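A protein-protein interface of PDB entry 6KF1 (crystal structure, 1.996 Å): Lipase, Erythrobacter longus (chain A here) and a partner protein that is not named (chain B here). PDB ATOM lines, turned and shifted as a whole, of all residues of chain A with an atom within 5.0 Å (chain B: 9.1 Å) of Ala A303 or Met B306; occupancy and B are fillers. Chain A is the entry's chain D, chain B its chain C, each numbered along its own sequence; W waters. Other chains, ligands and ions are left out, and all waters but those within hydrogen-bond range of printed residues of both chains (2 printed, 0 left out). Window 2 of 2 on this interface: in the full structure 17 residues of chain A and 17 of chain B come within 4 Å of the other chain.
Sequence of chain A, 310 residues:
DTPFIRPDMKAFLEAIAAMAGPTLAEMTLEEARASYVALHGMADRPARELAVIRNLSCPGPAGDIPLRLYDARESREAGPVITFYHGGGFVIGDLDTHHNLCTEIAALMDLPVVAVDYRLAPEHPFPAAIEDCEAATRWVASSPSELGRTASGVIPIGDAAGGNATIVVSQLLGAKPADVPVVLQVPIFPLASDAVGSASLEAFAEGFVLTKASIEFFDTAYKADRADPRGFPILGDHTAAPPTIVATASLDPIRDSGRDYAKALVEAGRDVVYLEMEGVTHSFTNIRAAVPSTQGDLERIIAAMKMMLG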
ATOM      1  N   VAL A 273     -16.688  34.016  19.668  1.00  0.00           N
ATOM      2  CA  VAL A 273     -17.911  33.840  20.449  1.00  0.00           C
ATOM      3  C   VAL A 273     -18.936  34.780  19.798  1.00  0.00           C
ATOM      4  O   VAL A 273     -18.606  36.025  19.680  1.00  0.00           O
ATOM      5  CB  VAL A 273     -17.657  34.208  21.901  1.00  0.00           C
ATOM      6  CG1 VAL A 273     -18.951  34.104  22.688  1.00  0.00           C
ATOM      7  CG2 VAL A 273     -16.540  33.358  22.512  1.00  0.00           C
ATOM      8  N   GLU A 299     -23.253  41.651  31.286  1.00  0.00           N
ATOM      9  CA  GLU A 299     -22.579  40.668  32.158  1.00  0.00           C
ATOM     10  C   GLU A 299     -22.230  39.393  31.356  1.00  0.00           C
ATOM     11  O   GLU A 299     -21.165  38.802  31.620  1.00  0.00           O
ATOM     12  CB  GLU A 299     -23.420  40.435  33.394  1.00  0.00           C
ATOM     13  CG  GLU A 299     -23.289  41.586  34.341  1.00  0.00           C
ATOM     14  CD  GLU A 299     -24.280  41.565  35.470  1.00  0.00           C
ATOM     15  OE1 GLU A 299     -25.201  40.714  35.477  1.00  0.00           O
ATOM     16  OE2 GLU A 299     -24.107  42.394  36.316  1.00  0.00           O
ATOM     17  N   ARG A 300     -23.060  39.008  30.393  1.00  0.00           N
ATOM     18  CA  ARG A 300     -22.735  37.849  29.498  1.00  0.00           C
ATOM     19  C   ARG A 300     -21.494  38.176  28.672  1.00  0.00           C
ATOM     20  O   ARG A 300     -20.666  37.242  28.493  1.00  0.00           O
ATOM     21  CB  ARG A 300     -23.910  37.456  28.616  1.00  0.00           C
ATOM     22  CG  ARG A 300     -25.087  36.953  29.445  1.00  0.00           C
ATOM     23  CD  ARG A 300     -26.194  36.582  28.489  1.00  0.00           C
ATOM     24  NE  ARG A 300     -25.748  35.514  27.601  1.00  0.00           N
ATOM     25  CZ  ARG A 300     -26.252  35.246  26.408  1.00  0.00           C
ATOM     26  NH1 ARG A 300     -27.249  35.984  25.917  1.00  0.00           N
ATOM     27  NH2 ARG A 300     -25.792  34.186  25.743  1.00  0.00           N
ATOM     28  N   ILE A 301     -21.366  39.406  28.178  1.00  0.00           N
ATOM     29  CA  ILE A 301     -20.181  39.814  27.376  1.00  0.00           C
ATOM     30  C   ILE A 301     -18.940  39.732  28.262  1.00  0.00           C
ATOM     31  O   ILE A 301     -17.928  39.116  27.829  1.00  0.00           O
ATOM     32  CB  ILE A 301     -20.320  41.200  26.737  1.00  0.00           C
ATOM     33  CG1 ILE A 301     -21.483  41.224  25.749  1.00  0.00           C
ATOM     34  CG2 ILE A 301     -19.014  41.636  26.073  1.00  0.00           C
ATOM     35  CD1 ILE A 301     -21.846  42.604  25.291  1.00  0.00           C
ATOM     36  N   ILE A 302     -19.036  40.237  29.473  1.00  0.00           N
ATOM     37  CA  ILE A 302     -17.946  40.156  30.470  1.00  0.00           C
ATOM     38  C   ILE A 302     -17.540  38.685  30.702  1.00  0.00           C
ATOM     39  O   ILE A 302     -16.296  38.409  30.730  1.00  0.00           O
ATOM     40  CB  ILE A 302     -18.374  40.843  31.779  1.00  0.00           C
ATOM     41  CG1 ILE A 302     -18.624  42.345  31.609  1.00  0.00           C
ATOM     42  CG2 ILE A 302     -17.379  40.551  32.890  1.00  0.00           C
ATOM     43  CD1 ILE A 302     -17.419  43.145  31.216  1.00  0.00           C
ATOM     44  N   ALA A 303     -18.486  37.779  30.934  1.00  0.00           N
ATOM     45  CA  ALA A 303     -18.200  36.351  31.209  1.00  0.00           C
ATOM     46  C   ALA A 303     -17.476  35.756  30.003  1.00  0.00           C
ATOM     47  O   ALA A 303     -16.497  34.973  30.190  1.00  0.00           O
ATOM     48  CB  ALA A 303     -19.460  35.573  31.547  1.00  0.00           C
ATOM     49  N   ALA A 304     -17.890  36.100  28.788  1.00  0.00           N
ATOM     50  CA  ALA A 304     -17.214  35.628  27.564  1.00  0.00           C
ATOM     51  C   ALA A 304     -15.786  36.180  27.476  1.00  0.00           C
ATOM     52  O   ALA A 304     -14.897  35.459  27.026  1.00  0.00           O
ATOM     53  CB  ALA A 304     -18.008  35.971  26.331  1.00  0.00           C
ATOM     54  N   MET A 305     -15.578  37.444  27.793  1.00  0.00           N
ATOM     55  CA  MET A 305     -14.228  38.047  27.826  1.00  0.00           C
ATOM     56  C   MET A 305     -13.322  37.297  28.801  1.00  0.00           C
ATOM     57  O   MET A 305     -12.197  36.988  28.407  1.00  0.00           O
ATOM     58  CB  MET A 305     -14.301  39.539  28.168  1.00  0.00           C
ATOM     59  CG  MET A 305     -14.946  40.327  27.068  1.00  0.00           C
ATOM     60  SD  MET A 305     -15.317  42.082  27.593  1.00  0.00           S
ATOM     61  CE  MET A 305     -13.669  42.697  27.918  1.00  0.00           C
ATOM     62  N   LYS A 306     -13.772  37.016  30.019  1.00  0.00           N
ATOM     63  CA  LYS A 306     -12.965  36.314  31.034  1.00  0.00           C
ATOM     64  C   LYS A 306     -12.614  34.911  30.510  1.00  0.00           C
ATOM     65  O   LYS A 306     -11.446  34.534  30.580  1.00  0.00           O
ATOM     66  CB  LYS A 306     -13.720  36.257  32.367  1.00  0.00           C
ATOM     67  CG  LYS A 306     -13.893  37.612  33.074  1.00  0.00           C
ATOM     68  CD  LYS A 306     -14.726  37.467  34.318  1.00  0.00           C
ATOM     69  CE  LYS A 306     -15.049  38.742  35.056  1.00  0.00           C
ATOM     70  NZ  LYS A 306     -13.905  39.090  35.902  1.00  0.00           N
ATOM     71  N   MET A 307     -13.585  34.202  29.930  1.00  0.00           N
ATOM     72  CA  MET A 307     -13.348  32.854  29.367  1.00  0.00           C
ATOM     73  C   MET A 307     -12.313  32.968  28.220  1.00  0.00           C
ATOM     74  O   MET A 307     -11.307  32.224  28.281  1.00  0.00           O
ATOM     75  CB  MET A 307     -14.671  32.241  28.914  1.00  0.00           C
ATOM     76  CG  MET A 307     -14.514  30.858  28.273  1.00  0.00           C
ATOM     77  SD  MET A 307     -14.199  30.848  26.552  1.00  0.00           S
ATOM     78  CE  MET A 307     -15.758  31.324  25.829  1.00  0.00           C
ATOM     79  N   MET B 108     -15.992  19.001  34.587  1.00  0.00           N
ATOM     80  CA  MET B 108     -17.278  19.742  34.597  1.00  0.00           C
ATOM     81  C   MET B 108     -17.954  19.649  35.965  1.00  0.00           C
ATOM     82  O   MET B 108     -18.856  20.462  36.242  1.00  0.00           O
ATOM     83  CB  MET B 108     -18.255  19.240  33.524  1.00  0.00           C
ATOM     84  CG  MET B 108     -17.856  19.626  32.171  1.00  0.00           C
ATOM     85  SD  MET B 108     -17.803  21.423  31.940  1.00  0.00           S
ATOM     86  CE  MET B 108     -19.460  21.974  32.325  1.00  0.00           C
ATOM     87  N   LEU B 183     -27.500  23.150  26.234  1.00  0.00           N
ATOM     88  CA  LEU B 183     -26.168  23.401  25.614  1.00  0.00           C
ATOM     89  C   LEU B 183     -25.888  22.163  24.765  1.00  0.00           C
ATOM     90  O   LEU B 183     -26.201  21.053  25.234  1.00  0.00           O
ATOM     91  CB  LEU B 183     -25.086  23.546  26.704  1.00  0.00           C
ATOM     92  CG  LEU B 183     -23.650  23.713  26.167  1.00  0.00           C
ATOM     93  CD1 LEU B 183     -23.525  24.954  25.297  1.00  0.00           C
ATOM     94  CD2 LEU B 183     -22.669  23.768  27.316  1.00  0.00           C
ATOM     95  N   PRO B 242     -27.931  26.845  22.725  1.00  0.00           N
ATOM     96  CA  PRO B 242     -26.597  27.409  22.830  1.00  0.00           C
ATOM     97  C   PRO B 242     -25.573  26.331  22.475  1.00  0.00           C
ATOM     98  O   PRO B 242     -25.818  25.200  22.861  1.00  0.00           O
ATOM     99  CB  PRO B 242     -26.477  27.730  24.308  1.00  0.00           C
ATOM    100  CG  PRO B 242     -27.919  27.965  24.757  1.00  0.00           C
ATOM    101  CD  PRO B 242     -28.690  26.930  23.982  1.00  0.00           C
ATOM    102  N   THR B 243     -24.574  26.689  21.672  1.00  0.00           N
ATOM    103  CA  THR B 243     -23.698  25.701  21.030  1.00  0.00           C
ATOM    104  C   THR B 243     -22.243  26.058  21.289  1.00  0.00           C
ATOM    105  O   THR B 243     -21.833  27.271  21.150  1.00  0.00           O
ATOM    106  CB  THR B 243     -24.012  25.612  19.536  1.00  0.00           C
ATOM    107  OG1 THR B 243     -25.370  25.180  19.460  1.00  0.00           O
ATOM    108  CG2 THR B 243     -23.077  24.629  18.856  1.00  0.00           C
ATOM    109  N   ILE B 244     -21.443  25.034  21.532  1.00  0.00           N
ATOM    110  CA  ILE B 244     -19.976  25.138  21.362  1.00  0.00           C
ATOM    111  C   ILE B 244     -19.563  24.183  20.240  1.00  0.00           C
ATOM    112  O   ILE B 244     -19.756  23.008  20.405  1.00  0.00           O
ATOM    113  CB  ILE B 244     -19.249  24.827  22.664  1.00  0.00           C
ATOM    114  CG1 ILE B 244     -19.666  25.819  23.732  1.00  0.00           C
ATOM    115  CG2 ILE B 244     -17.740  24.805  22.451  1.00  0.00           C
ATOM    116  CD1 ILE B 244     -19.464  25.294  25.094  1.00  0.00           C
ATOM    117  N   ASP B 270     -26.639  31.679  19.543  1.00  0.00           N
ATOM    118  CA  ASP B 270     -25.404  31.856  20.330  1.00  0.00           C
ATOM    119  C   ASP B 270     -24.470  30.659  20.055  1.00  0.00           C
ATOM    120  O   ASP B 270     -24.892  29.506  20.248  1.00  0.00           O
ATOM    121  CB  ASP B 270     -25.753  32.009  21.796  1.00  0.00           C
ATOM    122  CG  ASP B 270     -26.551  33.272  22.123  1.00  0.00           C
ATOM    123  OD1 ASP B 270     -26.655  34.192  21.271  1.00  0.00           O
ATOM    124  OD2 ASP B 270     -27.049  33.294  23.194  1.00  0.00           O
ATOM    125  N   VAL B 271     -23.216  30.944  19.722  1.00  0.00           N
ATOM    126  CA  VAL B 271     -22.249  29.865  19.398  1.00  0.00           C
ATOM    127  C   VAL B 271     -20.858  30.358  19.738  1.00  0.00           C
ATOM    128  O   VAL B 271     -20.535  31.524  19.450  1.00  0.00           O
ATOM    129  CB  VAL B 271     -22.379  29.401  17.937  1.00  0.00           C
ATOM    130  CG1 VAL B 271     -22.303  30.531  16.943  1.00  0.00           C
ATOM    131  CG2 VAL B 271     -21.343  28.326  17.599  1.00  0.00           C
ATOM    132  N   VAL B 272     -20.086  29.467  20.371  1.00  0.00           N
ATOM    133  CA  VAL B 272     -18.617  29.564  20.506  1.00  0.00           C
ATOM    134  C   VAL B 272     -17.999  28.662  19.450  1.00  0.00           C
ATOM    135  O   VAL B 272     -18.296  27.442  19.456  1.00  0.00           O
ATOM    136  CB  VAL B 272     -18.184  29.127  21.900  1.00  0.00           C
ATOM    137  CG1 VAL B 272     -16.657  29.231  22.036  1.00  0.00           C
ATOM    138  CG2 VAL B 272     -18.925  29.911  22.983  1.00  0.00           C
ATOM    139  N   TYR B 273     -17.182  29.238  18.598  1.00  0.00           N
ATOM    140  CA  TYR B 273     -16.447  28.502  17.561  1.00  0.00           C
ATOM    141  C   TYR B 273     -14.976  28.509  17.976  1.00  0.00           C
ATOM    142  O   TYR B 273     -14.368  29.587  18.034  1.00  0.00           O
ATOM    143  CB  TYR B 273     -16.644  29.070  16.167  1.00  0.00           C
ATOM    144  CG  TYR B 273     -15.882  28.249  15.151  1.00  0.00           C
ATOM    145  CD1 TYR B 273     -16.285  26.967  14.831  1.00  0.00           C
ATOM    146  CD2 TYR B 273     -14.677  28.696  14.637  1.00  0.00           C
ATOM    147  CE1 TYR B 273     -15.574  26.173  13.939  1.00  0.00           C
ATOM    148  CE2 TYR B 273     -13.925  27.901  13.791  1.00  0.00           C
ATOM    149  CZ  TYR B 273     -14.363  26.627  13.460  1.00  0.00           C
ATOM    150  OH  TYR B 273     -13.639  25.849  12.626  1.00  0.00           O
ATOM    151  N   LEU B 274     -14.447  27.330  18.307  1.00  0.00           N
ATOM    152  CA  LEU B 274     -13.014  27.135  18.635  1.00  0.00           C
ATOM    153  C   LEU B 274     -12.397  26.176  17.627  1.00  0.00           C
ATOM    154  O   LEU B 274     -12.834  25.002  17.547  1.00  0.00           O
ATOM    155  CB  LEU B 274     -12.834  26.563  20.041  1.00  0.00           C
ATOM    156  CG  LEU B 274     -13.521  27.335  21.171  1.00  0.00           C
ATOM    157  CD1 LEU B 274     -13.267  26.672  22.490  1.00  0.00           C
ATOM    158  CD2 LEU B 274     -13.057  28.782  21.208  1.00  0.00           C
ATOM    159  N   GLU B 298      -9.404  21.295  27.788  1.00  0.00           N
ATOM    160  CA  GLU B 298      -9.650  22.277  28.874  1.00  0.00           C
ATOM    161  C   GLU B 298     -10.259  23.582  28.328  1.00  0.00           C
ATOM    162  O   GLU B 298     -11.109  24.127  29.050  1.00  0.00           O
ATOM    163  CB  GLU B 298      -8.374  22.505  29.678  1.00  0.00           C
ATOM    164  CG  GLU B 298      -8.069  21.332  30.556  1.00  0.00           C
ATOM    165  CD  GLU B 298      -6.646  21.289  31.105  1.00  0.00           C
ATOM    166  OE1 GLU B 298      -5.804  22.149  30.714  1.00  0.00           O
ATOM    167  OE2 GLU B 298      -6.403  20.373  31.868  1.00  0.00           O
ATOM    168  N   ARG B 299      -9.922  24.016  27.107  1.00  0.00           N
ATOM    169  CA  ARG B 299     -10.584  25.203  26.509  1.00  0.00           C
ATOM    170  C   ARG B 299     -12.074  24.937  26.247  1.00  0.00           C
ATOM    171  O   ARG B 299     -12.923  25.866  26.466  1.00  0.00           O
ATOM    172  CB  ARG B 299      -9.909  25.651  25.229  1.00  0.00           C
ATOM    173  CG  ARG B 299      -8.495  26.141  25.494  1.00  0.00           C
ATOM    174  CD  ARG B 299      -7.870  26.579  24.212  1.00  0.00           C
ATOM    175  NE  ARG B 299      -8.669  27.664  23.661  1.00  0.00           N
ATOM    176  CZ  ARG B 299      -8.656  28.030  22.389  1.00  0.00           C
ATOM    177  NH1 ARG B 299      -7.891  27.383  21.521  1.00  0.00           N
ATOM    178  NH2 ARG B 299      -9.371  29.080  21.999  1.00  0.00           N
ATOM    179  N   ILE B 300     -12.401  23.741  25.764  1.00  0.00           N
ATOM    180  CA  ILE B 300     -13.815  23.309  25.546  1.00  0.00           C
ATOM    181  C   ILE B 300     -14.545  23.329  26.882  1.00  0.00           C
ATOM    182  O   ILE B 300     -15.660  23.892  26.953  1.00  0.00           O
ATOM    183  CB  ILE B 300     -13.913  21.926  24.865  1.00  0.00           C
ATOM    184  CG1 ILE B 300     -13.232  21.970  23.503  1.00  0.00           C
ATOM    185  CG2 ILE B 300     -15.361  21.474  24.762  1.00  0.00           C
ATOM    186  CD1 ILE B 300     -13.229  20.587  22.847  1.00  0.00           C
ATOM    187  N   ILE B 301     -13.936  22.782  27.915  1.00  0.00           N
ATOM    188  CA  ILE B 301     -14.524  22.749  29.285  1.00  0.00           C
ATOM    189  C   ILE B 301     -14.817  24.183  29.796  1.00  0.00           C
ATOM    190  O   ILE B 301     -15.940  24.423  30.291  1.00  0.00           O
ATOM    191  CB  ILE B 301     -13.582  22.017  30.246  1.00  0.00           C
ATOM    192  CG1 ILE B 301     -13.424  20.528  29.906  1.00  0.00           C
ATOM    193  CG2 ILE B 301     -14.007  22.255  31.703  1.00  0.00           C
ATOM    194  CD1 ILE B 301     -14.670  19.716  30.061  1.00  0.00           C
ATOM    195  N   ALA B 302     -13.858  25.091  29.680  1.00  0.00           N
ATOM    196  CA  ALA B 302     -14.019  26.508  30.075  1.00  0.00           C
ATOM    197  C   ALA B 302     -15.172  27.136  29.259  1.00  0.00           C
ATOM    198  O   ALA B 302     -15.990  27.865  29.843  1.00  0.00           O
ATOM    199  CB  ALA B 302     -12.714  27.228  29.866  1.00  0.00           C
ATOM    200  N   ALA B 303     -15.261  26.861  27.950  1.00  0.00           N
ATOM    201  CA  ALA B 303     -16.368  27.407  27.117  1.00  0.00           C
ATOM    202  C   ALA B 303     -17.701  26.859  27.631  1.00  0.00           C
ATOM    203  O   ALA B 303     -18.707  27.618  27.641  1.00  0.00           O
ATOM    204  CB  ALA B 303     -16.141  27.093  25.669  1.00  0.00           C
ATOM    205  N   MET B 304     -17.733  25.583  28.028  1.00  0.00           N
ATOM    206  CA  MET B 304     -18.969  24.904  28.497  1.00  0.00           C
ATOM    207  C   MET B 304     -19.428  25.568  29.798  1.00  0.00           C
ATOM    208  O   MET B 304     -20.625  25.854  29.938  1.00  0.00           O
ATOM    209  CB  MET B 304     -18.767  23.400  28.711  1.00  0.00           C
ATOM    210  CG  MET B 304     -18.641  22.659  27.419  1.00  0.00           C
ATOM    211  SD  MET B 304     -18.108  20.943  27.657  1.00  0.00           S
ATOM    212  CE  MET B 304     -19.408  20.199  28.621  1.00  0.00           C
ATOM    213  N   LYS B 305     -18.503  25.828  30.697  1.00  0.00           N
ATOM    214  CA  LYS B 305     -18.827  26.445  31.994  1.00  0.00           C
ATOM    215  C   LYS B 305     -19.323  27.859  31.744  1.00  0.00           C
ATOM    216  O   LYS B 305     -20.305  28.197  32.443  1.00  0.00           O
ATOM    217  CB  LYS B 305     -17.656  26.473  32.957  1.00  0.00           C
ATOM    218  CG  LYS B 305     -17.119  25.128  33.376  1.00  0.00           C
ATOM    219  CD  LYS B 305     -16.005  25.318  34.381  1.00  0.00           C
ATOM    220  CE  LYS B 305     -15.326  24.039  34.795  1.00  0.00           C
ATOM    221  NZ  LYS B 305     -16.202  23.276  35.702  1.00  0.00           N
ATOM    222  N   MET B 306     -18.731  28.587  30.788  1.00  0.00           N
ATOM    223  CA  MET B 306     -19.126  29.998  30.511  1.00  0.00           C
ATOM    224  C   MET B 306     -20.544  29.948  29.919  1.00  0.00           C
ATOM    225  O   MET B 306     -21.426  30.702  30.416  1.00  0.00           O
ATOM    226  CB  MET B 306     -18.130  30.703  29.583  1.00  0.00           C
ATOM    227  CG  MET B 306     -18.482  32.135  29.187  1.00  0.00           C
ATOM    228  SD  MET B 306     -19.490  32.218  27.761  1.00  0.00           S
ATOM    229  CE  MET B 306     -18.415  31.927  26.376  1.00  0.00           C
ATOM    230  N   MET B 307     -20.815  29.045  28.975  1.00  0.00           N
ATOM    231  CA  MET B 307     -22.125  29.000  28.269  1.00  0.00           C
ATOM    232  C   MET B 307     -23.235  28.465  29.175  1.00  0.00           C
ATOM    233  O   MET B 307     -24.364  28.916  28.974  1.00  0.00           O
ATOM    234  CB  MET B 307     -22.030  28.199  26.980  1.00  0.00           C
ATOM    235  CG  MET B 307     -21.172  28.890  25.970  1.00  0.00           C
ATOM    236  SD  MET B 307     -21.851  30.428  25.355  1.00  0.00           S
ATOM    237  CE  MET B 307     -22.995  29.785  24.130  1.00  0.00           C
ATOM    238  N   LEU B 308     -22.921  27.702  30.230  1.00  0.00           N
ATOM    239  CA  LEU B 308     -23.927  27.275  31.226  1.00  0.00           C
ATOM    240  C   LEU B 308     -24.167  28.372  32.293  1.00  0.00           C
ATOM    241  O   LEU B 308     -25.125  28.215  32.986  1.00  0.00           O
ATOM    242  CB  LEU B 308     -23.476  25.989  31.917  1.00  0.00           C
ATOM    243  CG  LEU B 308     -23.547  24.734  31.057  1.00  0.00           C
ATOM    244  CD1 LEU B 308     -22.849  23.553  31.764  1.00  0.00           C
ATOM    245  CD2 LEU B 308     -24.996  24.374  30.720  1.00  0.00           C
ATOM    246  N   GLY B 309     -23.297  29.370  32.501  1.00  0.00           N
ATOM    247  CA  GLY B 309     -23.573  30.591  33.316  1.00  0.00           C
ATOM    248  C   GLY B 309     -23.578  30.282  34.817  1.00  0.00           C
ATOM    249  O   GLY B 309     -22.942  29.314  35.213  1.00  0.00           O
HETATM  250  O   HOH W   1     -21.195  34.221  28.295  1.00  0.00           O
HETATM  251  O   HOH W   2     -28.788  35.231  23.426  1.00  0.00           O
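The side-chain carboxylate of Asp B270 lies within salt-bridge range of the guanidinium group of Arg A300, 3.0 Å away.
The backbone carbonyl oxygen of Asp B270 is in hydrogen-bond range of the backbone NH of Thr B243, 3.2 Å away.
Among the printed residues, pairs that only touch across the chains: Val A273 with Val B271, Ala A303 with Met B306, Met A307 with Ala B302 and Met A307 with Met B306.
Of the printed residues of chain B, Val A273 touches Val B271 (3.6 Å).
Of the printed residues of chain B, Arg A300 touches Asp B270.
Printed residues of chain B within 4 Å of Met A307: Ala B302 (3.7 Å) and Met B306 (2.8 Å).
Printed residues of chain A within 4 Å of Val B271: Val A273.
Of the printed residues of chain A, Ala B302 touches Met A307.
Of chain A, only Ala A303 and Met A307 come within 4 Å of Met B306.
The nearest residue of chain B that does not touch Ala A303 is Gly B309 (6.7 Å).
Printed residues of chain A that touch a printed residue of chain B: Val A273, Arg A300, Ala A303 and Met A307.
Along chain A the printed residues that touch a printed residue of chain B span positions 273 to 307.
Of the 22 printed residues of chain B, 4 touch a printed residue of chain A.
Hydrophobic or aromatic side chains of chain B that line the printed part of chain A: Met B306.
Along chain B the printed residues that touch a printed residue of chain A span positions 270 to 306.
Water W2 lies within hydrogen-bond range of the side-chain carboxylate of Asp B270 (2.6 Å) and the guanidinium group of Arg A300 (3.0 Å).
Water W1 lies within hydrogen-bond range of SD of Met B306 and O of Arg A300.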
